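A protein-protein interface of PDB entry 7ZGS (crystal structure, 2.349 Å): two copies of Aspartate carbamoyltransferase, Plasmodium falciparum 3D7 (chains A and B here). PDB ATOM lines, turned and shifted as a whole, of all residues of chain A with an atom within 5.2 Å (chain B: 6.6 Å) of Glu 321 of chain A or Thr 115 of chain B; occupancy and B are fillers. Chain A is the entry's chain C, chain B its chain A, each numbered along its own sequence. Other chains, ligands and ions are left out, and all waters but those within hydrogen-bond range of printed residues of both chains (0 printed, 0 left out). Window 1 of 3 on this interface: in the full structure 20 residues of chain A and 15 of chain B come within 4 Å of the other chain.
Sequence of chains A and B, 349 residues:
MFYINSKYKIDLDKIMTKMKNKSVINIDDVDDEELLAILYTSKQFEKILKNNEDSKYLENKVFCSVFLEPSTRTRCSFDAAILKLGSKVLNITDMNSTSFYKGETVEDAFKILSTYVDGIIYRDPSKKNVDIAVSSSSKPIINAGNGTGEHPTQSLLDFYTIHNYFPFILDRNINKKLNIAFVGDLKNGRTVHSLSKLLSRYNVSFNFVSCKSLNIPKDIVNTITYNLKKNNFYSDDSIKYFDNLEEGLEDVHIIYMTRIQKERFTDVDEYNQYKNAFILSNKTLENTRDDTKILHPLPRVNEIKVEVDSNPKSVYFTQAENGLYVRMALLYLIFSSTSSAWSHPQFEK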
ATOM      1  N   LYS A  50     -23.105  -3.190   6.753  1.00  0.00           N
ATOM      2  CA  LYS A  50     -21.735  -2.646   6.572  1.00  0.00           C
ATOM      3  C   LYS A  50     -20.744  -3.424   7.461  1.00  0.00           C
ATOM      4  O   LYS A  50     -19.570  -3.479   7.086  1.00  0.00           O
ATOM      5  CB  LYS A  50     -21.690  -1.137   6.825  1.00  0.00           C
ATOM      6  CG  LYS A  50     -22.422  -0.303   5.785  1.00  0.00           C
ATOM      7  CD  LYS A  50     -22.262   1.210   5.935  1.00  0.00           C
ATOM      8  CE  LYS A  50     -22.643   1.902   4.638  1.00  0.00           C
ATOM      9  NZ  LYS A  50     -22.428   3.373   4.639  1.00  0.00           N
ATOM     10  N   PHE A 317     -25.164   7.580  -5.480  1.00  0.00           N
ATOM     11  CA  PHE A 317     -24.972   6.105  -5.438  1.00  0.00           C
ATOM     12  C   PHE A 317     -25.211   5.607  -4.005  1.00  0.00           C
ATOM     13  O   PHE A 317     -25.830   4.536  -3.853  1.00  0.00           O
ATOM     14  CB  PHE A 317     -23.622   5.679  -6.008  1.00  0.00           C
ATOM     15  CG  PHE A 317     -23.467   5.966  -7.477  1.00  0.00           C
ATOM     16  CD1 PHE A 317     -24.223   5.285  -8.415  1.00  0.00           C
ATOM     17  CD2 PHE A 317     -22.588   6.937  -7.922  1.00  0.00           C
ATOM     18  CE1 PHE A 317     -24.073   5.555  -9.768  1.00  0.00           C
ATOM     19  CE2 PHE A 317     -22.440   7.194  -9.278  1.00  0.00           C
ATOM     20  CZ  PHE A 317     -23.178   6.500 -10.201  1.00  0.00           C
ATOM     21  N   THR A 318     -24.789   6.352  -2.986  1.00  0.00           N
ATOM     22  CA  THR A 318     -25.096   6.007  -1.575  1.00  0.00           C
ATOM     23  C   THR A 318     -26.633   6.022  -1.398  1.00  0.00           C
ATOM     24  O   THR A 318     -27.185   5.155  -0.665  1.00  0.00           O
ATOM     25  CB  THR A 318     -24.302   6.906  -0.619  1.00  0.00           C
ATOM     26  OG1 THR A 318     -22.902   6.757  -0.926  1.00  0.00           O
ATOM     27  CG2 THR A 318     -24.562   6.592   0.840  1.00  0.00           C
ATOM     28  N   GLN A 319     -27.307   6.926  -2.111  1.00  0.00           N
ATOM     29  CA  GLN A 319     -28.787   7.143  -2.083  1.00  0.00           C
ATOM     30  C   GLN A 319     -29.483   5.873  -2.555  1.00  0.00           C
ATOM     31  O   GLN A 319     -30.275   5.345  -1.806  1.00  0.00           O
ATOM     32  CB  GLN A 319     -29.133   8.336  -2.974  1.00  0.00           C
ATOM     33  CG  GLN A 319     -30.602   8.700  -3.044  1.00  0.00           C
ATOM     34  CD  GLN A 319     -30.854   9.755  -4.104  1.00  0.00           C
ATOM     35  OE1 GLN A 319     -29.937  10.301  -4.725  1.00  0.00           O
ATOM     36  NE2 GLN A 319     -32.114  10.013  -4.355  1.00  0.00           N
ATOM     37  N   ALA A 320     -29.201   5.434  -3.772  1.00  0.00           N
ATOM     38  CA  ALA A 320     -29.648   4.144  -4.352  1.00  0.00           C
ATOM     39  C   ALA A 320     -29.309   2.985  -3.386  1.00  0.00           C
ATOM     40  O   ALA A 320     -30.195   2.207  -3.034  1.00  0.00           O
ATOM     41  CB  ALA A 320     -29.021   3.991  -5.700  1.00  0.00           C
ATOM     42  N   GLU A 321     -28.072   2.898  -2.909  1.00  0.00           N
ATOM     43  CA  GLU A 321     -27.671   1.922  -1.871  1.00  0.00           C
ATOM     44  C   GLU A 321     -28.663   1.985  -0.696  1.00  0.00           C
ATOM     45  O   GLU A 321     -29.135   0.942  -0.274  1.00  0.00           O
ATOM     46  CB  GLU A 321     -26.226   2.176  -1.466  1.00  0.00           C
ATOM     47  CG  GLU A 321     -25.754   1.299  -0.331  1.00  0.00           C
ATOM     48  CD  GLU A 321     -24.382   1.687   0.234  1.00  0.00           C
ATOM     49  OE1 GLU A 321     -23.830   2.797  -0.084  1.00  0.00           O
ATOM     50  OE2 GLU A 321     -23.902   0.950   1.068  1.00  0.00           O
ATOM     51  N   ASN A 322     -28.982   3.166  -0.200  1.00  0.00           N
ATOM     52  CA  ASN A 322     -29.879   3.352   0.983  1.00  0.00           C
ATOM     53  C   ASN A 322     -31.295   2.795   0.765  1.00  0.00           C
ATOM     54  O   ASN A 322     -31.966   2.499   1.775  1.00  0.00           O
ATOM     55  CB  ASN A 322     -30.066   4.819   1.351  1.00  0.00           C
ATOM     56  CG  ASN A 322     -28.822   5.417   1.963  1.00  0.00           C
ATOM     57  OD1 ASN A 322     -28.047   4.726   2.624  1.00  0.00           O
ATOM     58  ND2 ASN A 322     -28.679   6.716   1.798  1.00  0.00           N
ATOM     59  N   GLY A 323     -31.750   2.730  -0.479  1.00  0.00           N
ATOM     60  CA  GLY A 323     -32.987   2.023  -0.849  1.00  0.00           C
ATOM     61  C   GLY A 323     -33.059   0.625  -0.240  1.00  0.00           C
ATOM     62  O   GLY A 323     -34.158   0.210   0.130  1.00  0.00           O
ATOM     63  N   LEU A 324     -31.936  -0.093  -0.153  1.00  0.00           N
ATOM     64  CA  LEU A 324     -31.907  -1.456   0.418  1.00  0.00           C
ATOM     65  C   LEU A 324     -32.303  -1.334   1.886  1.00  0.00           C
ATOM     66  O   LEU A 324     -33.240  -2.032   2.301  1.00  0.00           O
ATOM     67  CB  LEU A 324     -30.519  -2.089   0.255  1.00  0.00           C
ATOM     68  CG  LEU A 324     -30.325  -3.485   0.860  1.00  0.00           C
ATOM     69  CD1 LEU A 324     -31.419  -4.447   0.388  1.00  0.00           C
ATOM     70  CD2 LEU A 324     -28.916  -4.029   0.512  1.00  0.00           C
ATOM     71  N   TYR A 325     -31.644  -0.454   2.645  1.00  0.00           N
ATOM     72  CA  TYR A 325     -31.818  -0.395   4.116  1.00  0.00           C
ATOM     73  C   TYR A 325     -33.245   0.063   4.454  1.00  0.00           C
ATOM     74  O   TYR A 325     -33.831  -0.381   5.449  1.00  0.00           O
ATOM     75  CB  TYR A 325     -30.788   0.559   4.709  1.00  0.00           C
ATOM     76  CG  TYR A 325     -29.393   0.306   4.211  1.00  0.00           C
ATOM     77  CD1 TYR A 325     -28.881  -0.982   4.085  1.00  0.00           C
ATOM     78  CD2 TYR A 325     -28.562   1.359   3.900  1.00  0.00           C
ATOM     79  CE1 TYR A 325     -27.572  -1.205   3.675  1.00  0.00           C
ATOM     80  CE2 TYR A 325     -27.267   1.155   3.462  1.00  0.00           C
ATOM     81  CZ  TYR A 325     -26.766  -0.131   3.357  1.00  0.00           C
ATOM     82  OH  TYR A 325     -25.491  -0.294   2.903  1.00  0.00           O
ATOM     83  N   PHE B 110     -23.992  -1.448 -12.570  1.00  0.00           N
ATOM     84  CA  PHE B 110     -23.289  -2.436 -11.715  1.00  0.00           C
ATOM     85  C   PHE B 110     -22.874  -1.757 -10.415  1.00  0.00           C
ATOM     86  O   PHE B 110     -22.815  -2.469  -9.378  1.00  0.00           O
ATOM     87  CB  PHE B 110     -22.149  -3.125 -12.459  1.00  0.00           C
ATOM     88  CG  PHE B 110     -22.614  -4.403 -13.100  1.00  0.00           C
ATOM     89  CD1 PHE B 110     -22.476  -5.609 -12.441  1.00  0.00           C
ATOM     90  CD2 PHE B 110     -23.297  -4.376 -14.301  1.00  0.00           C
ATOM     91  CE1 PHE B 110     -22.964  -6.777 -13.005  1.00  0.00           C
ATOM     92  CE2 PHE B 110     -23.761  -5.544 -14.870  1.00  0.00           C
ATOM     93  CZ  PHE B 110     -23.591  -6.741 -14.221  1.00  0.00           C
ATOM     94  N   LYS B 111     -22.665  -0.438 -10.445  1.00  0.00           N
ATOM     95  CA  LYS B 111     -22.341   0.344  -9.228  1.00  0.00           C
ATOM     96  C   LYS B 111     -23.559   0.265  -8.304  1.00  0.00           C
ATOM     97  O   LYS B 111     -23.390   0.049  -7.107  1.00  0.00           O
ATOM     98  CB  LYS B 111     -21.925   1.770  -9.614  1.00  0.00           C
ATOM     99  CG  LYS B 111     -21.317   2.586  -8.481  1.00  0.00           C
ATOM    100  CD  LYS B 111     -20.534   3.818  -8.916  1.00  0.00           C
ATOM    101  CE  LYS B 111     -19.757   4.398  -7.743  1.00  0.00           C
ATOM    102  NZ  LYS B 111     -18.824   3.394  -7.148  1.00  0.00           N
ATOM    103  N   ILE B 112     -24.755   0.349  -8.851  1.00  0.00           N
ATOM    104  CA  ILE B 112     -26.003   0.248  -8.028  1.00  0.00           C
ATOM    105  C   ILE B 112     -26.267  -1.204  -7.584  1.00  0.00           C
ATOM    106  O   ILE B 112     -26.482  -1.424  -6.404  1.00  0.00           O
ATOM    107  CB  ILE B 112     -27.209   0.782  -8.803  1.00  0.00           C
ATOM    108  CG1 ILE B 112     -27.034   2.261  -9.105  1.00  0.00           C
ATOM    109  CG2 ILE B 112     -28.479   0.483  -8.039  1.00  0.00           C
ATOM    110  CD1 ILE B 112     -27.868   2.733 -10.275  1.00  0.00           C
ATOM    111  N   LEU B 113     -26.355  -2.136  -8.522  1.00  0.00           N
ATOM    112  CA  LEU B 113     -26.844  -3.504  -8.241  1.00  0.00           C
ATOM    113  C   LEU B 113     -25.921  -4.145  -7.209  1.00  0.00           C
ATOM    114  O   LEU B 113     -26.423  -4.801  -6.287  1.00  0.00           O
ATOM    115  CB  LEU B 113     -26.844  -4.261  -9.560  1.00  0.00           C
ATOM    116  CG  LEU B 113     -27.244  -5.729  -9.489  1.00  0.00           C
ATOM    117  CD1 LEU B 113     -28.641  -5.916  -8.877  1.00  0.00           C
ATOM    118  CD2 LEU B 113     -27.167  -6.316 -10.899  1.00  0.00           C
ATOM    119  N   SER B 114     -24.617  -3.906  -7.363  1.00  0.00           N
ATOM    120  CA  SER B 114     -23.555  -4.439  -6.475  1.00  0.00           C
ATOM    121  C   SER B 114     -23.730  -3.923  -5.045  1.00  0.00           C
ATOM    122  O   SER B 114     -23.210  -4.598  -4.173  1.00  0.00           O
ATOM    123  CB  SER B 114     -22.149  -4.243  -7.008  1.00  0.00           C
ATOM    124  OG  SER B 114     -21.668  -2.919  -6.903  1.00  0.00           O
ATOM    125  N   THR B 115     -24.449  -2.825  -4.782  1.00  0.00           N
ATOM    126  CA  THR B 115     -24.790  -2.403  -3.398  1.00  0.00           C
ATOM    127  C   THR B 115     -25.960  -3.240  -2.824  1.00  0.00           C
ATOM    128  O   THR B 115     -26.162  -3.168  -1.589  1.00  0.00           O
ATOM    129  CB  THR B 115     -25.105  -0.901  -3.297  1.00  0.00           C
ATOM    130  OG1 THR B 115     -26.367  -0.537  -3.885  1.00  0.00           O
ATOM    131  CG2 THR B 115     -23.972  -0.077  -3.862  1.00  0.00           C
ATOM    132  N   TYR B 116     -26.702  -3.998  -3.635  1.00  0.00           N
ATOM    133  CA  TYR B 116     -27.930  -4.716  -3.176  1.00  0.00           C
ATOM    134  C   TYR B 116     -27.594  -6.147  -2.719  1.00  0.00           C
ATOM    135  O   TYR B 116     -28.388  -6.749  -1.948  1.00  0.00           O
ATOM    136  CB  TYR B 116     -28.994  -4.812  -4.280  1.00  0.00           C
ATOM    137  CG  TYR B 116     -29.617  -3.526  -4.759  1.00  0.00           C
ATOM    138  CD1 TYR B 116     -29.488  -2.333  -4.061  1.00  0.00           C
ATOM    139  CD2 TYR B 116     -30.398  -3.521  -5.905  1.00  0.00           C
ATOM    140  CE1 TYR B 116     -30.109  -1.157  -4.489  1.00  0.00           C
ATOM    141  CE2 TYR B 116     -31.014  -2.357  -6.351  1.00  0.00           C
ATOM    142  CZ  TYR B 116     -30.880  -1.171  -5.640  1.00  0.00           C
ATOM    143  OH  TYR B 116     -31.503  -0.038  -6.093  1.00  0.00           O
ATOM    144  N   VAL B 117     -26.475  -6.709  -3.186  1.00  0.00           N
ATOM    145  CA  VAL B 117     -26.214  -8.173  -3.122  1.00  0.00           C
ATOM    146  C   VAL B 117     -24.740  -8.405  -2.763  1.00  0.00           C
ATOM    147  O   VAL B 117     -23.931  -7.449  -2.936  1.00  0.00           O
ATOM    148  CB  VAL B 117     -26.553  -8.825  -4.469  1.00  0.00           C
ATOM    149  CG1 VAL B 117     -28.020  -8.663  -4.815  1.00  0.00           C
ATOM    150  CG2 VAL B 117     -25.684  -8.277  -5.596  1.00  0.00           C
ATOM    151  N   ILE B 120     -22.461 -11.251  -7.995  1.00  0.00           N
ATOM    152  CA  ILE B 120     -23.260 -11.209  -9.242  1.00  0.00           C
ATOM    153  C   ILE B 120     -22.757 -12.308 -10.169  1.00  0.00           C
ATOM    154  O   ILE B 120     -21.524 -12.426 -10.295  1.00  0.00           O
ATOM    155  CB  ILE B 120     -23.180  -9.821  -9.881  1.00  0.00           C
ATOM    156  CG1 ILE B 120     -23.763  -8.786  -8.924  1.00  0.00           C
ATOM    157  CG2 ILE B 120     -23.851  -9.841 -11.245  1.00  0.00           C
ATOM    158  CD1 ILE B 120     -23.443  -7.350  -9.255  1.00  0.00           C
ATOM    159  N   SER B 138     -18.680  -3.199  -6.773  1.00  0.00           N
ATOM    160  CA  SER B 138     -18.110  -3.272  -5.414  1.00  0.00           C
ATOM    161  C   SER B 138     -18.095  -4.734  -4.940  1.00  0.00           C
ATOM    162  O   SER B 138     -17.719  -4.971  -3.806  1.00  0.00           O
ATOM    163  CB  SER B 138     -18.964  -2.357  -4.550  1.00  0.00           C
ATOM    164  OG  SER B 138     -18.993  -2.743  -3.192  1.00  0.00           O
ATOM    165  N   LYS B 139     -18.597  -5.667  -5.752  1.00  0.00           N
ATOM    166  CA  LYS B 139     -18.736  -7.089  -5.352  1.00  0.00           C
ATOM    167  C   LYS B 139     -18.213  -8.025  -6.433  1.00  0.00           C
ATOM    168  O   LYS B 139     -18.160  -7.693  -7.614  1.00  0.00           O
ATOM    169  CB  LYS B 139     -20.177  -7.449  -5.008  1.00  0.00           C
ATOM    170  CG  LYS B 139     -20.778  -6.577  -3.921  1.00  0.00           C
ATOM    171  CD  LYS B 139     -20.213  -6.799  -2.527  1.00  0.00           C
ATOM    172  CE  LYS B 139     -20.591  -5.672  -1.581  1.00  0.00           C
ATOM    173  NZ  LYS B 139     -22.053  -5.363  -1.634  1.00  0.00           N
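OG of Ser 114 of chain B sits at hydrogen-bond distance from O of Lys 111 of chain B (3.4 Å). O of Ile 112 of chain B lies within hydrogen-bond range of OG1 of Thr 115 of chain B. OH of Tyr 325 of chain A sits at hydrogen-bond distance from OE2 of Glu 321 of chain A, at 2.7 Å.
Among the printed residues, pairs that only touch across the chains: Glu 321 of chain A with Thr 115 of chain B (3.4 Å), Leu 324 of chain A with Thr 115 of chain B (3.6 Å), Ala 320 of chain A with Tyr 116 of chain B (3.7 Å), Leu 324 of chain A with Tyr 116 of chain B (3.7 Å) and Phe 317 of chain A with Lys 111 of chain B (3.8 Å).
Glu 321 of chain A touches just one residue of chain B: Thr 115 (3.4 Å). Thr 115 of chain B touches just these residues of chain A: Glu 321 and Leu 324. Of the printed residues of chain A, Lys 111 of chain B touches Phe 317. Printed residues of chain B within 4 Å of Leu 324 of chain A: Thr 115 (3.6 Å) and Tyr 116 (3.7 Å). Of the printed residues of chain A, Tyr 116 of chain B touches Ala 320 (3.7 Å) and Leu 324 (3.7 Å). Printed residues of chain B within 4 Å of Ala 320 of chain A: Tyr 116. Gln 319 of chain A touches none of the printed residues of chain B. The nearest residue of chain B that does not touch Glu 321 of chain A is Tyr 116 of chain B (4.7 Å). The nearest residue of chain A that does not touch Thr 115 of chain B is Ala 320 of chain A (4.6 Å).
Hydrophobic or aromatic side chains of chain B that line the printed part of chain A: Tyr 116. Along chain B the printed residues that touch a printed residue of chain A span positions 111 to 116. Hydrophobic or aromatic side chains of chain A that line the printed part of chain B: Phe 317 and Leu 324. Along chain A the printed residues that touch a printed residue of chain B span positions 317 to 324. Among the printed residues, 5 pairs touch across the chains.
No position is printed for both chains. Of the 5 pairs that touch across the chains among the printed residues, none has its exchanged pair printed and touching as well.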
